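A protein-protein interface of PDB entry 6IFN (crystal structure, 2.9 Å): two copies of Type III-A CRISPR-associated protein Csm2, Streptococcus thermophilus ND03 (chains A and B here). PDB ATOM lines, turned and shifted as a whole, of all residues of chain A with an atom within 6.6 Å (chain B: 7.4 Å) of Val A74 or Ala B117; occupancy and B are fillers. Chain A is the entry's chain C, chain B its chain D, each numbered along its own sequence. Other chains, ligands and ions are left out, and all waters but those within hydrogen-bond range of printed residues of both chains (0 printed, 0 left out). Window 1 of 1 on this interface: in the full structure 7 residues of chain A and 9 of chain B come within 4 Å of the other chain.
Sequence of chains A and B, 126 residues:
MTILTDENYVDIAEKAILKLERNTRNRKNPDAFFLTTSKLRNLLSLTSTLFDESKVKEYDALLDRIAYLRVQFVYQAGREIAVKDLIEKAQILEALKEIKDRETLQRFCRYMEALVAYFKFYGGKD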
ATOM      1  N   LEU A  43       4.913  -6.555  27.372  1.00  0.00           N
ATOM      2  CA  LEU A  43       4.067  -5.936  26.370  1.00  0.00           C
ATOM      3  C   LEU A  43       2.692  -6.589  26.411  1.00  0.00           C
ATOM      4  O   LEU A  43       1.670  -5.914  26.532  1.00  0.00           O
ATOM      5  CB  LEU A  43       4.732  -6.174  25.006  1.00  0.00           C
ATOM      6  CG  LEU A  43       4.366  -5.263  23.839  1.00  0.00           C
ATOM      7  CD1 LEU A  43       4.591  -3.797  24.176  1.00  0.00           C
ATOM      8  CD2 LEU A  43       5.189  -5.653  22.627  1.00  0.00           C
ATOM      9  N   LEU A  69      -0.061   1.543  25.735  1.00  0.00           N
ATOM     10  CA  LEU A  69       0.215   0.353  24.906  1.00  0.00           C
ATOM     11  C   LEU A  69       1.087   0.746  23.698  1.00  0.00           C
ATOM     12  O   LEU A  69       2.160   0.189  23.489  1.00  0.00           O
ATOM     13  CB  LEU A  69      -1.100  -0.290  24.432  1.00  0.00           C
ATOM     14  CG  LEU A  69      -1.202  -1.819  24.538  1.00  0.00           C
ATOM     15  CD1 LEU A  69      -2.145  -2.389  23.494  1.00  0.00           C
ATOM     16  CD2 LEU A  69       0.153  -2.507  24.432  1.00  0.00           C
ATOM     17  N   ARG A  70       0.617   1.711  22.906  1.00  0.00           N
ATOM     18  CA  ARG A  70       1.288   2.119  21.689  1.00  0.00           C
ATOM     19  C   ARG A  70       2.754   2.421  21.996  1.00  0.00           C
ATOM     20  O   ARG A  70       3.680   1.916  21.322  1.00  0.00           O
ATOM     21  CB  ARG A  70       0.592   3.359  21.116  1.00  0.00           C
ATOM     22  CG  ARG A  70       1.333   4.074  19.994  1.00  0.00           C
ATOM     23  CD  ARG A  70       0.803   5.481  19.814  1.00  0.00           C
ATOM     24  NE  ARG A  70       1.174   6.043  18.517  1.00  0.00           N
ATOM     25  CZ  ARG A  70       0.391   6.827  17.790  1.00  0.00           C
ATOM     26  NH1 ARG A  70      -0.838   7.075  18.206  1.00  0.00           N
ATOM     27  NH2 ARG A  70       0.831   7.353  16.659  1.00  0.00           N
ATOM     28  N   VAL A  71       2.935   3.272  23.011  1.00  0.00           N
ATOM     29  CA  VAL A  71       4.248   3.722  23.458  1.00  0.00           C
ATOM     30  C   VAL A  71       5.146   2.493  23.638  1.00  0.00           C
ATOM     31  O   VAL A  71       6.135   2.347  22.903  1.00  0.00           O
ATOM     32  CB  VAL A  71       4.165   4.570  24.747  1.00  0.00           C
ATOM     33  CG1 VAL A  71       5.473   4.579  25.538  1.00  0.00           C
ATOM     34  CG2 VAL A  71       3.730   5.995  24.432  1.00  0.00           C
ATOM     35  N   GLN A  72       4.762   1.615  24.579  1.00  0.00           N
ATOM     36  CA  GLN A  72       5.512   0.446  24.919  1.00  0.00           C
ATOM     37  C   GLN A  72       5.858  -0.348  23.658  1.00  0.00           C
ATOM     38  O   GLN A  72       7.001  -0.775  23.496  1.00  0.00           O
ATOM     39  CB  GLN A  72       4.714  -0.456  25.844  1.00  0.00           C
ATOM     40  CG  GLN A  72       5.611  -1.361  26.668  1.00  0.00           C
ATOM     41  CD  GLN A  72       6.439  -0.561  27.632  1.00  0.00           C
ATOM     42  OE1 GLN A  72       6.016   0.502  28.090  1.00  0.00           O
ATOM     43  NE2 GLN A  72       7.626  -1.068  27.902  1.00  0.00           N
ATOM     44  N   PHE A  73       4.884  -0.488  22.748  1.00  0.00           N
ATOM     45  CA  PHE A  73       5.115  -1.229  21.523  1.00  0.00           C
ATOM     46  C   PHE A  73       6.313  -0.649  20.776  1.00  0.00           C
ATOM     47  O   PHE A  73       7.300  -1.365  20.551  1.00  0.00           O
ATOM     48  CB  PHE A  73       3.870  -1.272  20.636  1.00  0.00           C
ATOM     49  CG  PHE A  73       3.105  -2.571  20.743  1.00  0.00           C
ATOM     50  CD1 PHE A  73       3.585  -3.727  20.148  1.00  0.00           C
ATOM     51  CD2 PHE A  73       1.925  -2.642  21.468  1.00  0.00           C
ATOM     52  CE1 PHE A  73       2.893  -4.920  20.278  1.00  0.00           C
ATOM     53  CE2 PHE A  73       1.225  -3.833  21.582  1.00  0.00           C
ATOM     54  CZ  PHE A  73       1.714  -4.968  20.989  1.00  0.00           C
ATOM     55  N   VAL A  74       6.247   0.645  20.439  1.00  0.00           N
ATOM     56  CA  VAL A  74       7.350   1.265  19.687  1.00  0.00           C
ATOM     57  C   VAL A  74       8.648   1.161  20.514  1.00  0.00           C
ATOM     58  O   VAL A  74       9.685   0.744  19.986  1.00  0.00           O
ATOM     59  CB  VAL A  74       7.061   2.711  19.236  1.00  0.00           C
ATOM     60  CG1 VAL A  74       6.005   2.770  18.155  1.00  0.00           C
ATOM     61  CG2 VAL A  74       6.683   3.623  20.374  1.00  0.00           C
ATOM     62  N   TYR A  75       8.570   1.455  21.815  1.00  0.00           N
ATOM     63  CA  TYR A  75       9.744   1.399  22.673  1.00  0.00           C
ATOM     64  C   TYR A  75      10.418   0.033  22.527  1.00  0.00           C
ATOM     65  O   TYR A  75      11.615  -0.035  22.268  1.00  0.00           O
ATOM     66  CB  TYR A  75       9.394   1.730  24.125  1.00  0.00           C
ATOM     67  CG  TYR A  75      10.585   1.770  25.055  1.00  0.00           C
ATOM     68  CD1 TYR A  75      11.779   2.386  24.692  1.00  0.00           C
ATOM     69  CD2 TYR A  75      10.538   1.145  26.285  1.00  0.00           C
ATOM     70  CE1 TYR A  75      12.877   2.403  25.538  1.00  0.00           C
ATOM     71  CE2 TYR A  75      11.631   1.137  27.138  1.00  0.00           C
ATOM     72  CZ  TYR A  75      12.806   1.775  26.772  1.00  0.00           C
ATOM     73  OH  TYR A  75      13.866   1.750  27.643  1.00  0.00           O
ATOM     74  N   GLN A  76       9.646  -1.042  22.651  1.00  0.00           N
ATOM     75  CA  GLN A  76      10.232  -2.388  22.592  1.00  0.00           C
ATOM     76  C   GLN A  76      10.731  -2.658  21.168  1.00  0.00           C
ATOM     77  O   GLN A  76      11.774  -3.308  21.002  1.00  0.00           O
ATOM     78  CB  GLN A  76       9.274  -3.521  22.979  1.00  0.00           C
ATOM     79  CG  GLN A  76       8.664  -3.407  24.368  1.00  0.00           C
ATOM     80  CD  GLN A  76       9.721  -3.225  25.418  1.00  0.00           C
ATOM     81  OE1 GLN A  76      10.843  -3.680  25.256  1.00  0.00           O
ATOM     82  NE2 GLN A  76       9.357  -2.560  26.497  1.00  0.00           N
ATOM     83  N   ALA A  77       9.995  -2.155  20.165  1.00  0.00           N
ATOM     84  CA  ALA A  77      10.410  -2.333  18.781  1.00  0.00           C
ATOM     85  C   ALA A  77      11.727  -1.592  18.562  1.00  0.00           C
ATOM     86  O   ALA A  77      12.552  -2.019  17.775  1.00  0.00           O
ATOM     87  CB  ALA A  77       9.345  -1.882  17.821  1.00  0.00           C
ATOM     88  N   GLY A  78      11.913  -0.489  19.294  1.00  0.00           N
ATOM     89  CA  GLY A  78      13.178   0.238  19.331  1.00  0.00           C
ATOM     90  C   GLY A  78      14.298  -0.566  19.971  1.00  0.00           C
ATOM     91  O   GLY A  78      15.391  -0.571  19.477  1.00  0.00           O
ATOM     92  N   ARG A  79      14.011  -1.235  21.083  1.00  0.00           N
ATOM     93  CA  ARG A  79      15.040  -1.878  21.865  1.00  0.00           C
ATOM     94  C   ARG A  79      15.375  -3.282  21.341  1.00  0.00           C
ATOM     95  O   ARG A  79      16.469  -3.774  21.617  1.00  0.00           O
ATOM     96  CB  ARG A  79      14.618  -1.907  23.332  1.00  0.00           C
ATOM     97  CG  ARG A  79      15.025  -0.649  24.077  1.00  0.00           C
ATOM     98  CD  ARG A  79      14.511  -0.657  25.495  1.00  0.00           C
ATOM     99  NE  ARG A  79      14.553  -1.974  26.129  1.00  0.00           N
ATOM    100  CZ  ARG A  79      13.481  -2.646  26.544  1.00  0.00           C
ATOM    101  NH1 ARG A  79      12.273  -2.143  26.352  1.00  0.00           N
ATOM    102  NH2 ARG A  79      13.625  -3.804  27.159  1.00  0.00           N
ATOM    103  N   VAL A  83      11.455  -7.907  17.812  1.00  0.00           N
ATOM    104  CA  VAL A  83      10.201  -7.258  18.165  1.00  0.00           C
ATOM    105  C   VAL A  83       9.759  -6.367  16.997  1.00  0.00           C
ATOM    106  O   VAL A  83       8.632  -6.512  16.500  1.00  0.00           O
ATOM    107  CB  VAL A  83      10.287  -6.452  19.470  1.00  0.00           C
ATOM    108  CG1 VAL A  83       9.195  -5.395  19.552  1.00  0.00           C
ATOM    109  CG2 VAL A  83      10.220  -7.356  20.686  1.00  0.00           C
ATOM    110  N   ILE A  87       6.209  -6.576  14.947  1.00  0.00           N
ATOM    111  CA  ILE A  87       5.150  -5.576  14.925  1.00  0.00           C
ATOM    112  C   ILE A  87       5.120  -4.924  13.539  1.00  0.00           C
ATOM    113  O   ILE A  87       4.260  -4.089  13.284  1.00  0.00           O
ATOM    114  CB  ILE A  87       5.302  -4.536  16.050  1.00  0.00           C
ATOM    115  CG1 ILE A  87       6.214  -3.389  15.632  1.00  0.00           C
ATOM    116  CG2 ILE A  87       5.751  -5.156  17.363  1.00  0.00           C
ATOM    117  CD1 ILE A  87       6.068  -2.200  16.528  1.00  0.00           C
ATOM    118  N   LEU A  93       0.940  -1.791  14.890  1.00  0.00           N
ATOM    119  CA  LEU A  93       0.659  -0.391  15.263  1.00  0.00           C
ATOM    120  C   LEU A  93      -0.514   0.162  14.446  1.00  0.00           C
ATOM    121  O   LEU A  93      -1.373   0.829  15.003  1.00  0.00           O
ATOM    122  CB  LEU A  93       1.904   0.472  15.084  1.00  0.00           C
ATOM    123  CG  LEU A  93       3.185  -0.143  15.623  1.00  0.00           C
ATOM    124  CD1 LEU A  93       3.938  -0.881  14.511  1.00  0.00           C
ATOM    125  CD2 LEU A  93       4.032   0.940  16.264  1.00  0.00           C
ATOM    126  N   GLU B  14       5.556  12.057  18.088  1.00  0.00           N
ATOM    127  CA  GLU B  14       6.088  11.463  16.862  1.00  0.00           C
ATOM    128  C   GLU B  14       6.430  12.586  15.869  1.00  0.00           C
ATOM    129  O   GLU B  14       7.567  12.697  15.418  1.00  0.00           O
ATOM    130  CB  GLU B  14       5.075  10.478  16.272  1.00  0.00           C
ATOM    131  CG  GLU B  14       5.702   9.256  15.638  1.00  0.00           C
ATOM    132  CD  GLU B  14       4.752   8.380  14.849  1.00  0.00           C
ATOM    133  OE1 GLU B  14       3.604   8.782  14.681  1.00  0.00           O
ATOM    134  OE2 GLU B  14       5.164   7.307  14.398  1.00  0.00           O
ATOM    135  N   ILE B  17       9.510  14.080  16.618  1.00  0.00           N
ATOM    136  CA  ILE B  17      10.721  13.277  16.558  1.00  0.00           C
ATOM    137  C   ILE B  17      11.144  13.058  15.099  1.00  0.00           C
ATOM    138  O   ILE B  17      12.340  13.069  14.807  1.00  0.00           O
ATOM    139  CB  ILE B  17      10.538  11.957  17.333  1.00  0.00           C
ATOM    140  CG1 ILE B  17      10.813  12.159  18.827  1.00  0.00           C
ATOM    141  CG2 ILE B  17      11.363  10.820  16.744  1.00  0.00           C
ATOM    142  CD1 ILE B  17      12.255  12.415  19.174  1.00  0.00           C
ATOM    143  N   TYR B 111       4.378  12.446  28.153  1.00  0.00           N
ATOM    144  CA  TYR B 111       4.884  13.000  26.908  1.00  0.00           C
ATOM    145  C   TYR B 111       6.361  12.636  26.744  1.00  0.00           C
ATOM    146  O   TYR B 111       6.794  12.187  25.679  1.00  0.00           O
ATOM    147  CB  TYR B 111       4.665  14.513  26.850  1.00  0.00           C
ATOM    148  CG  TYR B 111       5.052  15.130  25.531  1.00  0.00           C
ATOM    149  CD1 TYR B 111       4.557  14.638  24.332  1.00  0.00           C
ATOM    150  CD2 TYR B 111       5.892  16.230  25.491  1.00  0.00           C
ATOM    151  CE1 TYR B 111       4.913  15.208  23.120  1.00  0.00           C
ATOM    152  CE2 TYR B 111       6.258  16.813  24.289  1.00  0.00           C
ATOM    153  CZ  TYR B 111       5.761  16.302  23.099  1.00  0.00           C
ATOM    154  OH  TYR B 111       6.104  16.884  21.911  1.00  0.00           O
ATOM    155  N   MET B 112       7.134  12.809  27.813  1.00  0.00           N
ATOM    156  CA  MET B 112       8.535  12.475  27.753  1.00  0.00           C
ATOM    157  C   MET B 112       8.667  10.999  27.362  1.00  0.00           C
ATOM    158  O   MET B 112       9.444  10.679  26.439  1.00  0.00           O
ATOM    159  CB  MET B 112       9.265  12.752  29.076  1.00  0.00           C
ATOM    160  CG  MET B 112       9.744  14.196  29.242  1.00  0.00           C
ATOM    161  SD  MET B 112      10.530  14.886  27.736  1.00  0.00           S
ATOM    162  CE  MET B 112      11.811  13.667  27.459  1.00  0.00           C
ATOM    163  N   GLU B 113       7.911  10.130  28.055  1.00  0.00           N
ATOM    164  CA  GLU B 113       7.951   8.696  27.827  1.00  0.00           C
ATOM    165  C   GLU B 113       7.790   8.447  26.319  1.00  0.00           C
ATOM    166  O   GLU B 113       8.529   7.665  25.710  1.00  0.00           O
ATOM    167  CB  GLU B 113       6.856   7.981  28.624  1.00  0.00           C
ATOM    168  N   ALA B 114       6.820   9.152  25.731  1.00  0.00           N
ATOM    169  CA  ALA B 114       6.420   8.922  24.344  1.00  0.00           C
ATOM    170  C   ALA B 114       7.555   9.314  23.401  1.00  0.00           C
ATOM    171  O   ALA B 114       7.885   8.577  22.467  1.00  0.00           O
ATOM    172  CB  ALA B 114       5.159   9.698  24.025  1.00  0.00           C
ATOM    173  N   LEU B 115       8.111  10.500  23.657  1.00  0.00           N
ATOM    174  CA  LEU B 115       9.206  11.035  22.862  1.00  0.00           C
ATOM    175  C   LEU B 115      10.325   9.996  22.787  1.00  0.00           C
ATOM    176  O   LEU B 115      10.816   9.700  21.694  1.00  0.00           O
ATOM    177  CB  LEU B 115       9.701  12.345  23.489  1.00  0.00           C
ATOM    178  CG  LEU B 115       8.823  13.574  23.240  1.00  0.00           C
ATOM    179  CD1 LEU B 115       9.276  14.740  24.113  1.00  0.00           C
ATOM    180  CD2 LEU B 115       8.852  13.935  21.759  1.00  0.00           C
ATOM    181  N   VAL B 116      10.690   9.445  23.954  1.00  0.00           N
ATOM    182  CA  VAL B 116      11.840   8.541  24.079  1.00  0.00           C
ATOM    183  C   VAL B 116      11.541   7.247  23.313  1.00  0.00           C
ATOM    184  O   VAL B 116      12.402   6.721  22.616  1.00  0.00           O
ATOM    185  CB  VAL B 116      12.186   8.235  25.548  1.00  0.00           C
ATOM    186  CG1 VAL B 116      13.354   7.265  25.636  1.00  0.00           C
ATOM    187  CG2 VAL B 116      12.464   9.493  26.361  1.00  0.00           C
ATOM    188  N   ALA B 117      10.308   6.750  23.458  1.00  0.00           N
ATOM    189  CA  ALA B 117       9.899   5.525  22.810  1.00  0.00           C
ATOM    190  C   ALA B 117      10.071   5.662  21.301  1.00  0.00           C
ATOM    191  O   ALA B 117      10.681   4.821  20.667  1.00  0.00           O
ATOM    192  CB  ALA B 117       8.479   5.206  23.177  1.00  0.00           C
ATOM    193  N   TYR B 118       9.532   6.745  20.741  1.00  0.00           N
ATOM    194  CA  TYR B 118       9.564   6.951  19.304  1.00  0.00           C
ATOM    195  C   TYR B 118      10.986   7.293  18.826  1.00  0.00           C
ATOM    196  O   TYR B 118      11.309   7.070  17.656  1.00  0.00           O
ATOM    197  CB  TYR B 118       8.521   7.993  18.897  1.00  0.00           C
ATOM    198  CG  TYR B 118       7.258   7.378  18.358  1.00  0.00           C
ATOM    199  CD1 TYR B 118       7.310   6.485  17.298  1.00  0.00           C
ATOM    200  CD2 TYR B 118       6.013   7.706  18.867  1.00  0.00           C
ATOM    201  CE1 TYR B 118       6.162   5.926  16.764  1.00  0.00           C
ATOM    202  CE2 TYR B 118       4.854   7.158  18.336  1.00  0.00           C
ATOM    203  CZ  TYR B 118       4.929   6.263  17.286  1.00  0.00           C
ATOM    204  OH  TYR B 118       3.796   5.711  16.762  1.00  0.00           O
ATOM    205  N   PHE B 119      11.818   7.829  19.728  1.00  0.00           N
ATOM    206  CA  PHE B 119      13.236   8.057  19.437  1.00  0.00           C
ATOM    207  C   PHE B 119      13.930   6.709  19.197  1.00  0.00           C
ATOM    208  O   PHE B 119      14.552   6.490  18.164  1.00  0.00           O
ATOM    209  CB  PHE B 119      13.920   8.860  20.554  1.00  0.00           C
ATOM    210  CG  PHE B 119      15.430   8.847  20.476  1.00  0.00           C
ATOM    211  CD1 PHE B 119      16.107   9.570  19.499  1.00  0.00           C
ATOM    212  CD2 PHE B 119      16.175   8.085  21.364  1.00  0.00           C
ATOM    213  CE1 PHE B 119      17.488   9.526  19.406  1.00  0.00           C
ATOM    214  CE2 PHE B 119      17.558   8.053  21.278  1.00  0.00           C
ATOM    215  CZ  PHE B 119      18.212   8.776  20.305  1.00  0.00           C
ATOM    216  N   LYS B 120      13.806   5.805  20.165  1.00  0.00           N
ATOM    217  CA  LYS B 120      14.436   4.504  20.075  1.00  0.00           C
ATOM    218  C   LYS B 120      13.878   3.729  18.868  1.00  0.00           C
ATOM    219  O   LYS B 120      14.610   2.968  18.202  1.00  0.00           O
ATOM    220  CB  LYS B 120      14.251   3.741  21.387  1.00  0.00           C
ATOM    221  CG  LYS B 120      15.156   4.205  22.518  1.00  0.00           C
ATOM    222  CD  LYS B 120      16.424   3.390  22.682  1.00  0.00           C
ATOM    223  CE  LYS B 120      17.341   3.416  21.478  1.00  0.00           C
ATOM    224  NZ  LYS B 120      18.336   2.320  21.538  1.00  0.00           N
ATOM    225  N   PHE B 121      12.587   3.919  18.572  1.00  0.00           N
ATOM    226  CA  PHE B 121      11.942   3.184  17.497  1.00  0.00           C
ATOM    227  C   PHE B 121      12.597   3.557  16.166  1.00  0.00           C
ATOM    228  O   PHE B 121      12.913   2.687  15.359  1.00  0.00           O
ATOM    229  CB  PHE B 121      10.437   3.476  17.449  1.00  0.00           C
ATOM    230  CG  PHE B 121       9.710   2.872  16.272  1.00  0.00           C
ATOM    231  CD1 PHE B 121       9.191   1.594  16.342  1.00  0.00           C
ATOM    232  CD2 PHE B 121       9.554   3.570  15.091  1.00  0.00           C
ATOM    233  CE1 PHE B 121       8.536   1.022  15.263  1.00  0.00           C
ATOM    234  CE2 PHE B 121       8.913   2.992  14.010  1.00  0.00           C
ATOM    235  CZ  PHE B 121       8.402   1.722  14.097  1.00  0.00           C
ATOM    236  N   TYR B 122      12.790   4.865  15.966  1.00  0.00           N
ATOM    237  CA  TYR B 122      13.142   5.416  14.669  1.00  0.00           C
ATOM    238  C   TYR B 122      14.663   5.427  14.437  1.00  0.00           C
ATOM    239  O   TYR B 122      15.119   6.060  13.484  1.00  0.00           O
ATOM    240  CB  TYR B 122      12.534   6.814  14.520  1.00  0.00           C
ATOM    241  CG  TYR B 122      11.149   6.811  13.928  1.00  0.00           C
ATOM    242  CD1 TYR B 122      10.937   6.287  12.663  1.00  0.00           C
ATOM    243  CD2 TYR B 122      10.057   7.333  14.610  1.00  0.00           C
ATOM    244  CE1 TYR B 122       9.676   6.266  12.091  1.00  0.00           C
ATOM    245  CE2 TYR B 122       8.789   7.311  14.056  1.00  0.00           C
ATOM    246  CZ  TYR B 122       8.601   6.800  12.782  1.00  0.00           C
ATOM    247  OH  TYR B 122       7.352   6.779  12.233  1.00  0.00           O
ATOM    248  N   GLY B 123      15.417   4.701  15.271  1.00  0.00           N
ATOM    249  CA  GLY B 123      16.825   4.386  15.011  1.00  0.00           C
ATOM    250  C   GLY B 123      17.774   5.178  15.883  1.00  0.00           C
ATOM    251  O   GLY B 123      18.923   5.272  15.550  1.00  0.00           O
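The side-chain carboxylate (OE2) of Glu B14 lies close to the side-chain hydroxyl (OH) of Tyr B118 (3.2 Å).
OH of Tyr B122 is in hydrogen-bond range of OE2 of Glu B14 (3.1 Å).
The side-chain carboxylate of Glu B14 is in salt-bridge range of the guanidinium group of Arg A70 (3.7 Å).
The guanidinium group of Arg A70 is in hydrogen-bond range of the side-chain hydroxyl of Tyr B118 (3.2 Å).
No position is printed for both chains.
CA of Ala B114 touches CG2 of Val A71 (3.98 Å).
O of Val A71 touches CB of Ala B117, 3.7 Å away.
Val A74 touches Ala B117 (CG2 to CB, 3.7 Å).
Tyr B118 touches Val A74.
Val A74 touches Phe B121 (CB to CD1, 3.8 Å).
Ala B117 touches Tyr A75 (CB to CB, 3.7 Å).
Phe B121 touches Ala A77 (CD1 to CB, 3.8 Å).
Lys B120 touches Gly A78 (O to CA, 3.3 Å).
Gly A78 touches Phe B121 (CA to CA, 3.7 Å).
Of the printed residues of chain B, Arg A70 touches Glu B14 and Tyr B118.
Printed residues of chain B within 4 Å of Val A71: Ala B114 (3.98 Å) and Ala B117 (3.7 Å).
Of chain B, only Ala B117 (3.7 Å), Tyr B118 (3.5 Å) and Phe B121 (3.8 Å) come within 4 Å of Val A74.
Of the printed residues of chain B, Tyr A75 touches Ala B117.
Printed residues of chain A within 4 Å of Ala B114: Val A71.
Ala B117 touches just these residues of chain A: Val A71, Val A74 and Tyr A75.
Of the printed residues of chain A, Phe B121 touches Val A74 (3.8 Å), Ala A77 (3.8 Å) and Gly A78 (3.7 Å).
Of the 15 printed residues of chain A, 6 touch a printed residue of chain B.
Hydrophobic or aromatic side chains of chain A within 4 Å of the printed part of chain B: Val A71, Val A74, Tyr A75 and Ala A77.
Printed residues of chain B that touch a printed residue of chain A: Glu B14, Ala B114, Ala B117, Tyr B118, Lys B120 and Phe B121.
Hydrophobic or aromatic side chains of chain B that line the printed part of chain A: Ala B114, Ala B117, Tyr B118 and Phe B121.
Among the printed residues, Asp or Glu carboxylates within 4 Å of a Lys or Arg side-chain nitrogen of the other chain: Arg A70 with Glu B14.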
